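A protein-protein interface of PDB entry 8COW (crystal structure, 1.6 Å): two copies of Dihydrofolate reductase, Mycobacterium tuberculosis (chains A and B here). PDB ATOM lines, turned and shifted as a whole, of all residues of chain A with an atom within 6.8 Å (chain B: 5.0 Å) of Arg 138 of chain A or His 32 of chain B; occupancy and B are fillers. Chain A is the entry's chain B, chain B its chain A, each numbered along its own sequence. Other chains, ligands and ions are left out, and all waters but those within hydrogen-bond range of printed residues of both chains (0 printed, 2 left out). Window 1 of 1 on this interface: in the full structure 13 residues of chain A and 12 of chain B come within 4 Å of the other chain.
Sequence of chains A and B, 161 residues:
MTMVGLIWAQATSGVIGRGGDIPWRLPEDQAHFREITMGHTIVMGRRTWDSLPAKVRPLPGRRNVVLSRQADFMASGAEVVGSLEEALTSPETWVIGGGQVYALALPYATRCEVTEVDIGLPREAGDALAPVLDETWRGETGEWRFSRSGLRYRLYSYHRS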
ATOM      1  N   ASP A 134      27.448  19.563  -0.103  1.00  0.00           N
ATOM      2  CA  ASP A 134      28.358  20.262  -1.040  1.00  0.00           C
ATOM      3  C   ASP A 134      27.628  20.678  -2.324  1.00  0.00           C
ATOM      4  O   ASP A 134      26.425  20.512  -2.470  1.00  0.00           O
ATOM      5  CB  ASP A 134      29.669  19.504  -1.185  1.00  0.00           C
ATOM      6  CG  ASP A 134      29.546  18.223  -1.946  1.00  0.00           C
ATOM      7  OD1 ASP A 134      28.607  18.090  -2.662  1.00  0.00           O
ATOM      8  OD2 ASP A 134      30.386  17.399  -1.799  1.00  0.00           O
ATOM      9  N   GLU A 135      28.367  21.138  -3.325  1.00  0.00           N
ATOM     10  CA  GLU A 135      27.614  21.646  -4.492  1.00  0.00           C
ATOM     11  C   GLU A 135      27.078  20.552  -5.409  1.00  0.00           C
ATOM     12  O   GLU A 135      26.363  20.892  -6.262  1.00  0.00           O
ATOM     13  CB  GLU A 135      28.193  22.922  -5.077  1.00  0.00           C
ATOM     14  CG  GLU A 135      27.248  24.087  -4.863  1.00  0.00           C
ATOM     15  CD  GLU A 135      26.989  24.450  -3.412  1.00  0.00           C
ATOM     16  OE1 GLU A 135      25.904  24.924  -3.112  1.00  0.00           O
ATOM     17  OE2 GLU A 135      27.893  24.271  -2.609  1.00  0.00           O
ATOM     18  N   THR A 136      27.377  19.287  -5.188  1.00  0.00           N
ATOM     19  CA  THR A 136      26.760  18.239  -6.006  1.00  0.00           C
ATOM     20  C   THR A 136      25.248  18.125  -5.740  1.00  0.00           C
ATOM     21  O   THR A 136      24.587  17.596  -6.588  1.00  0.00           O
ATOM     22  CB  THR A 136      27.517  16.930  -5.830  1.00  0.00           C
ATOM     23  OG1 THR A 136      27.349  16.488  -4.497  1.00  0.00           O
ATOM     24  CG2 THR A 136      28.987  17.085  -6.110  1.00  0.00           C
ATOM     25  N   TRP A 137      24.733  18.625  -4.610  1.00  0.00           N
ATOM     26  CA  TRP A 137      23.327  18.470  -4.283  1.00  0.00           C
ATOM     27  C   TRP A 137      22.499  19.585  -4.903  1.00  0.00           C
ATOM     28  O   TRP A 137      22.826  20.768  -4.771  1.00  0.00           O
ATOM     29  CB  TRP A 137      23.121  18.442  -2.770  1.00  0.00           C
ATOM     30  CG  TRP A 137      23.732  17.237  -2.137  1.00  0.00           C
ATOM     31  CD1 TRP A 137      24.989  17.129  -1.643  1.00  0.00           C
ATOM     32  CD2 TRP A 137      23.119  15.959  -1.962  1.00  0.00           C
ATOM     33  NE1 TRP A 137      25.198  15.872  -1.144  1.00  0.00           N
ATOM     34  CE2 TRP A 137      24.058  15.133  -1.328  1.00  0.00           C
ATOM     35  CE3 TRP A 137      21.860  15.435  -2.273  1.00  0.00           C
ATOM     36  CZ2 TRP A 137      23.791  13.807  -1.009  1.00  0.00           C
ATOM     37  CZ3 TRP A 137      21.591  14.120  -1.936  1.00  0.00           C
ATOM     38  CH2 TRP A 137      22.552  13.323  -1.313  1.00  0.00           C
ATOM     39  N   ARG A 138      21.427  19.189  -5.578  1.00  0.00           N
ATOM     40  CA  ARG A 138      20.420  20.085  -6.116  1.00  0.00           C
ATOM     41  C   ARG A 138      19.205  20.042  -5.202  1.00  0.00           C
ATOM     42  O   ARG A 138      18.714  18.958  -4.868  1.00  0.00           O
ATOM     43  CB  ARG A 138      20.046  19.660  -7.535  1.00  0.00           C
ATOM     44  CG  ARG A 138      21.208  19.740  -8.527  1.00  0.00           C
ATOM     45  CD  ARG A 138      20.836  19.196  -9.917  1.00  0.00           C
ATOM     46  NE  ARG A 138      19.436  19.402 -10.284  1.00  0.00           N
ATOM     47  CZ  ARG A 138      18.988  20.442 -10.982  1.00  0.00           C
ATOM     48  NH1 ARG A 138      19.829  21.379 -11.405  1.00  0.00           N
ATOM     49  NH2 ARG A 138      17.696  20.540 -11.264  1.00  0.00           N
ATOM     50  N   GLY A 139      18.730  21.211  -4.793  1.00  0.00           N
ATOM     51  CA  GLY A 139      17.674  21.312  -3.799  1.00  0.00           C
ATOM     52  C   GLY A 139      16.443  22.004  -4.351  1.00  0.00           C
ATOM     53  O   GLY A 139      16.553  22.963  -5.117  1.00  0.00           O
ATOM     54  N   GLU A 140      15.275  21.507  -3.960  1.00  0.00           N
ATOM     55  CA  GLU A 140      14.000  22.139  -4.274  1.00  0.00           C
ATOM     56  C   GLU A 140      13.315  22.465  -2.952  1.00  0.00           C
ATOM     57  O   GLU A 140      13.059  21.564  -2.143  1.00  0.00           O
ATOM     58  CB  GLU A 140      13.124  21.242  -5.155  1.00  0.00           C
ATOM     59  CG  GLU A 140      13.871  20.488  -6.271  1.00  0.00           C
ATOM     60  CD  GLU A 140      14.432  21.396  -7.367  1.00  0.00           C
ATOM     61  OE1 GLU A 140      15.539  21.108  -7.871  1.00  0.00           O
ATOM     62  OE2 GLU A 140      13.781  22.401  -7.721  1.00  0.00           O
ATOM     63  N   SER A 157      13.703  18.991  -0.605  1.00  0.00           N
ATOM     64  CA  SER A 157      14.047  17.750  -1.279  1.00  0.00           C
ATOM     65  C   SER A 157      15.370  18.013  -1.995  1.00  0.00           C
ATOM     66  O   SER A 157      15.423  18.826  -2.921  1.00  0.00           O
ATOM     67  CB  SER A 157      12.949  17.346  -2.259  1.00  0.00           C
ATOM     68  OG  SER A 157      11.797  16.900  -1.563  1.00  0.00           O
ATOM     69  N   TYR A 158      16.444  17.386  -1.533  1.00  0.00           N
ATOM     70  CA  TYR A 158      17.744  17.469  -2.189  1.00  0.00           C
ATOM     71  C   TYR A 158      18.007  16.176  -2.939  1.00  0.00           C
ATOM     72  O   TYR A 158      17.717  15.086  -2.439  1.00  0.00           O
ATOM     73  CB  TYR A 158      18.869  17.698  -1.183  1.00  0.00           C
ATOM     74  CG  TYR A 158      18.838  19.037  -0.501  1.00  0.00           C
ATOM     75  CD1 TYR A 158      18.218  19.198   0.736  1.00  0.00           C
ATOM     76  CD2 TYR A 158      19.475  20.128  -1.060  1.00  0.00           C
ATOM     77  CE1 TYR A 158      18.206  20.418   1.371  1.00  0.00           C
ATOM     78  CE2 TYR A 158      19.473  21.350  -0.436  1.00  0.00           C
ATOM     79  CZ  TYR A 158      18.836  21.495   0.778  1.00  0.00           C
ATOM     80  OH  TYR A 158      18.847  22.723   1.390  1.00  0.00           O
ATOM     81  N   HIS A 159      18.560  16.303  -4.142  1.00  0.00           N
ATOM     82  CA  HIS A 159      18.785  15.165  -5.015  1.00  0.00           C
ATOM     83  C   HIS A 159      20.113  15.340  -5.731  1.00  0.00           C
ATOM     84  O   HIS A 159      20.590  16.462  -5.930  1.00  0.00           O
ATOM     85  CB  HIS A 159      17.652  14.999  -6.046  1.00  0.00           C
ATOM     86  N   ARG A 160      20.711  14.213  -6.098  1.00  0.00           N
ATOM     87  CA  ARG A 160      21.917  14.204  -6.905  1.00  0.00           C
ATOM     88  C   ARG A 160      21.983  12.847  -7.580  1.00  0.00           C
ATOM     89  O   ARG A 160      21.552  11.838  -7.011  1.00  0.00           O
ATOM     90  CB  ARG A 160      23.178  14.482  -6.072  1.00  0.00           C
ATOM     91  CG  ARG A 160      23.636  13.337  -5.167  1.00  0.00           C
ATOM     92  CD  ARG A 160      24.989  13.653  -4.538  1.00  0.00           C
ATOM     93  NE  ARG A 160      25.414  12.649  -3.546  1.00  0.00           N
ATOM     94  CZ  ARG A 160      26.596  12.655  -2.932  1.00  0.00           C
ATOM     95  NH1 ARG A 160      27.476  13.606  -3.195  1.00  0.00           N
ATOM     96  NH2 ARG A 160      26.895  11.724  -2.041  1.00  0.00           N
ATOM     97  N   SER A 161      22.465  12.843  -8.808  1.00  0.00           N
ATOM     98  CA  SER A 161      22.708  11.596  -9.491  1.00  0.00           C
ATOM     99  C   SER A 161      23.790  10.779  -8.758  1.00  0.00           C
ATOM    100  O   SER A 161      23.691   9.550  -8.647  1.00  0.00           O
ATOM    101  CB  SER A 161      23.113  11.886 -10.930  1.00  0.00           C
ATOM    102  OG  SER A 161      24.481  12.242 -10.989  1.00  0.00           O
ATOM    103  OXT SER A 161      24.783  11.312  -8.249  1.00  0.00           O
ATOM    104  N   ILE B   7       8.141  10.187 -14.449  1.00  0.00           N
ATOM    105  CA  ILE B   7       8.577  11.577 -14.498  1.00  0.00           C
ATOM    106  C   ILE B   7       8.001  12.213 -15.765  1.00  0.00           C
ATOM    107  O   ILE B   7       8.135  11.661 -16.868  1.00  0.00           O
ATOM    108  CB  ILE B   7      10.121  11.685 -14.449  1.00  0.00           C
ATOM    109  CG1 ILE B   7      10.586  13.144 -14.391  1.00  0.00           C
ATOM    110  CG2 ILE B   7      10.792  10.936 -15.609  1.00  0.00           C
ATOM    111  CD1 ILE B   7      11.988  13.309 -13.734  1.00  0.00           C
ATOM    112  N   GLU B  28      15.324  24.443 -17.184  1.00  0.00           N
ATOM    113  CA  GLU B  28      15.439  23.951 -15.822  1.00  0.00           C
ATOM    114  C   GLU B  28      14.787  22.591 -15.679  1.00  0.00           C
ATOM    115  O   GLU B  28      15.243  21.760 -14.881  1.00  0.00           O
ATOM    116  CB  GLU B  28      14.800  24.944 -14.848  1.00  0.00           C
ATOM    117  CG  GLU B  28      15.574  26.241 -14.731  1.00  0.00           C
ATOM    118  CD  GLU B  28      15.162  27.259 -15.779  1.00  0.00           C
ATOM    119  OE1 GLU B  28      15.622  28.418 -15.682  1.00  0.00           O
ATOM    120  OE2 GLU B  28      14.364  26.906 -16.691  1.00  0.00           O
ATOM    121  N   ASP B  29      13.714  22.345 -16.428  1.00  0.00           N
ATOM    122  CA  ASP B  29      13.052  21.051 -16.335  1.00  0.00           C
ATOM    123  C   ASP B  29      13.913  19.953 -16.944  1.00  0.00           C
ATOM    124  O   ASP B  29      13.975  18.834 -16.418  1.00  0.00           O
ATOM    125  CB  ASP B  29      11.697  21.095 -17.032  1.00  0.00           C
ATOM    126  CG  ASP B  29      11.076  19.719 -17.156  1.00  0.00           C
ATOM    127  OD1 ASP B  29      10.726  19.124 -16.101  1.00  0.00           O
ATOM    128  OD2 ASP B  29      11.015  19.194 -18.306  1.00  0.00           O
ATOM    129  N   GLN B  30      14.569  20.251 -18.066  1.00  0.00           N
ATOM    130  CA  GLN B  30      15.501  19.297 -18.666  1.00  0.00           C
ATOM    131  C   GLN B  30      16.629  18.941 -17.705  1.00  0.00           C
ATOM    132  O   GLN B  30      16.981  17.767 -17.556  1.00  0.00           O
ATOM    133  CB  GLN B  30      16.059  19.860 -19.972  1.00  0.00           C
ATOM    134  CG  GLN B  30      17.004  18.901 -20.708  1.00  0.00           C
ATOM    135  CD  GLN B  30      17.369  19.384 -22.095  1.00  0.00           C
ATOM    136  OE1 GLN B  30      16.607  20.109 -22.731  1.00  0.00           O
ATOM    137  NE2 GLN B  30      18.563  19.013 -22.560  1.00  0.00           N
ATOM    138  N   ALA B  31      17.225  19.946 -17.053  1.00  0.00           N
ATOM    139  CA  ALA B  31      18.263  19.668 -16.064  1.00  0.00           C
ATOM    140  C   ALA B  31      17.714  18.827 -14.913  1.00  0.00           C
ATOM    141  O   ALA B  31      18.367  17.879 -14.453  1.00  0.00           O
ATOM    142  CB  ALA B  31      18.874  20.982 -15.561  1.00  0.00           C
ATOM    143  N   HIS B  32      16.499  19.147 -14.453  1.00  0.00           N
ATOM    144  CA  HIS B  32      15.820  18.325 -13.456  1.00  0.00           C
ATOM    145  C   HIS B  32      15.653  16.890 -13.942  1.00  0.00           C
ATOM    146  O   HIS B  32      15.936  15.932 -13.211  1.00  0.00           O
ATOM    147  CB  HIS B  32      14.457  18.967 -13.133  1.00  0.00           C
ATOM    148  CG  HIS B  32      13.604  18.193 -12.175  1.00  0.00           C
ATOM    149  ND1 HIS B  32      12.435  17.576 -12.566  1.00  0.00           N
ATOM    150  CD2 HIS B  32      13.723  17.961 -10.848  1.00  0.00           C
ATOM    151  CE1 HIS B  32      11.874  16.995 -11.521  1.00  0.00           C
ATOM    152  NE2 HIS B  32      12.638  17.211 -10.466  1.00  0.00           N
ATOM    153  N   PHE B  33      15.162  16.729 -15.169  1.00  0.00           N
ATOM    154  CA  PHE B  33      14.946  15.403 -15.727  1.00  0.00           C
ATOM    155  C   PHE B  33      16.253  14.641 -15.834  1.00  0.00           C
ATOM    156  O   PHE B  33      16.313  13.435 -15.560  1.00  0.00           O
ATOM    157  CB  PHE B  33      14.283  15.545 -17.100  1.00  0.00           C
ATOM    158  CG  PHE B  33      14.279  14.282 -17.909  1.00  0.00           C
ATOM    159  CD1 PHE B  33      15.278  14.041 -18.848  1.00  0.00           C
ATOM    160  CD2 PHE B  33      13.294  13.335 -17.725  1.00  0.00           C
ATOM    161  CE1 PHE B  33      15.267  12.877 -19.587  1.00  0.00           C
ATOM    162  CE2 PHE B  33      13.282  12.166 -18.460  1.00  0.00           C
ATOM    163  CZ  PHE B  33      14.272  11.939 -19.388  1.00  0.00           C
ATOM    164  N   ARG B  34      17.307  15.324 -16.250  1.00  0.00           N
ATOM    165  CA  ARG B  34      18.591  14.650 -16.421  1.00  0.00           C
ATOM    166  C   ARG B  34      19.134  14.161 -15.086  1.00  0.00           C
ATOM    167  O   ARG B  34      19.618  13.025 -14.980  1.00  0.00           O
ATOM    168  CB  ARG B  34      19.564  15.608 -17.093  1.00  0.00           C
ATOM    169  CG  ARG B  34      20.959  15.065 -17.253  1.00  0.00           C
ATOM    170  CD  ARG B  34      21.849  16.110 -17.884  1.00  0.00           C
ATOM    171  NE  ARG B  34      23.238  15.653 -17.950  1.00  0.00           N
ATOM    172  CZ  ARG B  34      24.102  15.776 -16.946  1.00  0.00           C
ATOM    173  NH1 ARG B  34      25.348  15.342 -17.080  1.00  0.00           N
ATOM    174  NH2 ARG B  34      23.713  16.319 -15.796  1.00  0.00           N
ATOM    175  N   GLU B  35      19.031  14.997 -14.053  1.00  0.00           N
ATOM    176  CA  GLU B  35      19.528  14.647 -12.724  1.00  0.00           C
ATOM    177  C   GLU B  35      18.780  13.462 -12.124  1.00  0.00           C
ATOM    178  O   GLU B  35      19.397  12.571 -11.524  1.00  0.00           O
ATOM    179  CB  GLU B  35      19.418  15.860 -11.801  1.00  0.00           C
ATOM    180  CG  GLU B  35      20.314  15.815 -10.562  1.00  0.00           C
ATOM    181  CD  GLU B  35      21.796  16.052 -10.878  1.00  0.00           C
ATOM    182  OE1 GLU B  35      22.665  15.475 -10.174  1.00  0.00           O
ATOM    183  OE2 GLU B  35      22.093  16.825 -11.816  1.00  0.00           O
ATOM    184  N   ILE B  36      17.458  13.419 -12.285  1.00  0.00           N
ATOM    185  CA  ILE B  36      16.671  12.360 -11.650  1.00  0.00           C
ATOM    186  C   ILE B  36      16.872  11.024 -12.376  1.00  0.00           C
ATOM    187  O   ILE B  36      16.939   9.960 -11.744  1.00  0.00           O
ATOM    188  CB  ILE B  36      15.188  12.765 -11.602  1.00  0.00           C
ATOM    189  CG1 ILE B  36      14.975  13.807 -10.509  1.00  0.00           C
ATOM    190  CG2 ILE B  36      14.281  11.570 -11.284  1.00  0.00           C
ATOM    191  CD1 ILE B  36      13.536  14.217 -10.390  1.00  0.00           C
ATOM    192  N   GLU B 113       7.371  12.268 -10.314  1.00  0.00           N
ATOM    193  CA  GLU B 113       8.050  13.551 -10.226  1.00  0.00           C
ATOM    194  C   GLU B 113       7.492  14.408 -11.361  1.00  0.00           C
ATOM    195  O   GLU B 113       7.724  14.117 -12.542  1.00  0.00           O
ATOM    196  CB  GLU B 113       9.571  13.388 -10.329  1.00  0.00           C
ATOM    197  CG  GLU B 113      10.178  12.676  -9.117  1.00  0.00           C
ATOM    198  CD  GLU B 113      10.163  13.528  -7.833  1.00  0.00           C
ATOM    199  OE1 GLU B 113      10.269  12.937  -6.732  1.00  0.00           O
ATOM    200  OE2 GLU B 113      10.035  14.774  -7.911  1.00  0.00           O
ATOM    201  N   THR B 115       6.590  18.134 -13.242  1.00  0.00           N
ATOM    202  CA  THR B 115       6.816  19.552 -13.490  1.00  0.00           C
ATOM    203  C   THR B 115       5.527  20.152 -14.038  1.00  0.00           C
ATOM    204  O   THR B 115       5.013  19.695 -15.063  1.00  0.00           O
ATOM    205  CB  THR B 115       7.960  19.767 -14.484  1.00  0.00           C
ATOM    206  OG1 THR B 115       9.177  19.210 -13.953  1.00  0.00           O
ATOM    207  CG2 THR B 115       8.156  21.248 -14.739  1.00  0.00           C
ATOM    208  N   LEU B 155       7.395  22.260  -9.162  1.00  0.00           N
ATOM    209  CA  LEU B 155       7.728  20.845  -9.091  1.00  0.00           C
ATOM    210  C   LEU B 155       6.921  20.175  -7.996  1.00  0.00           C
ATOM    211  O   LEU B 155       6.781  20.728  -6.903  1.00  0.00           O
ATOM    212  CB  LEU B 155       9.215  20.660  -8.789  1.00  0.00           C
ATOM    213  CG  LEU B 155      10.153  21.228  -9.848  1.00  0.00           C
ATOM    214  CD1 LEU B 155      11.604  21.003  -9.431  1.00  0.00           C
ATOM    215  CD2 LEU B 155       9.867  20.604 -11.196  1.00  0.00           C
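Arg 138 of chain A touches two residues of chain B.
Of the printed residues of chain B, Arg 160 of chain A touches Glu 35 (3.6 Å).
Printed residues of chain B within 4 Å of Ser 161 of chain A: Glu 35.
Of chain A, only Arg 138 (3.6 Å) comes within 4 Å of His 32 of chain B.
The nearest residue of chain B that does not touch Arg 138 of chain A is Ala 31 of chain B (4.03 Å).
The nearest residue of chain A that does not touch His 32 of chain B is Glu 140 of chain A (4.7 Å).
The nearest printed residue of chain A that does not touch Glu 35 of chain B is Thr 136 of chain A (4.6 Å).
The side-chain carboxylate (OE1) of Glu 35 of chain B is in hydrogen-bond range of the backbone NH (N) of Ser 161 of chain A (3.0 Å).
No position is printed for both chains.
The side-chain hydroxyl of Thr 136 of chain A is in hydrogen-bond range of the guanidinium group of Arg 160 of chain A.
The backbone carbonyl oxygen (O) of Ser 157 of chain A sits at hydrogen-bond distance from the backbone NH (N) of Glu 140 of chain A (2.9 Å).
N of His 159 of chain A sits at hydrogen-bond distance from O of Arg 138 of chain A, 2.8 Å away.
Of the 13 printed residues of chain B, 3 touch a printed residue of chain A.
Hydrophobic or aromatic side chains of chain B within 4 Å of the printed part of chain A: Leu 155.
Of the 12 printed residues of chain A, 4 touch a printed residue of chain B.
Printed residues of chain A that touch a printed residue of chain B: Arg 138, Glu 140, Arg 160 and Ser 161.
Along chain A the printed residues that touch a printed residue of chain B span positions 138 to 161.
Among the printed residues, 5 pairs touch across the chains.
Among the printed residues, merely in contact across the chains: Glu 140 of chain A with Leu 155 of chain B, Arg 138 of chain A with Glu 35 of chain B, Arg 160 of chain A with Glu 35 of chain B and Arg 138 of chain A with His 32 of chain B.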
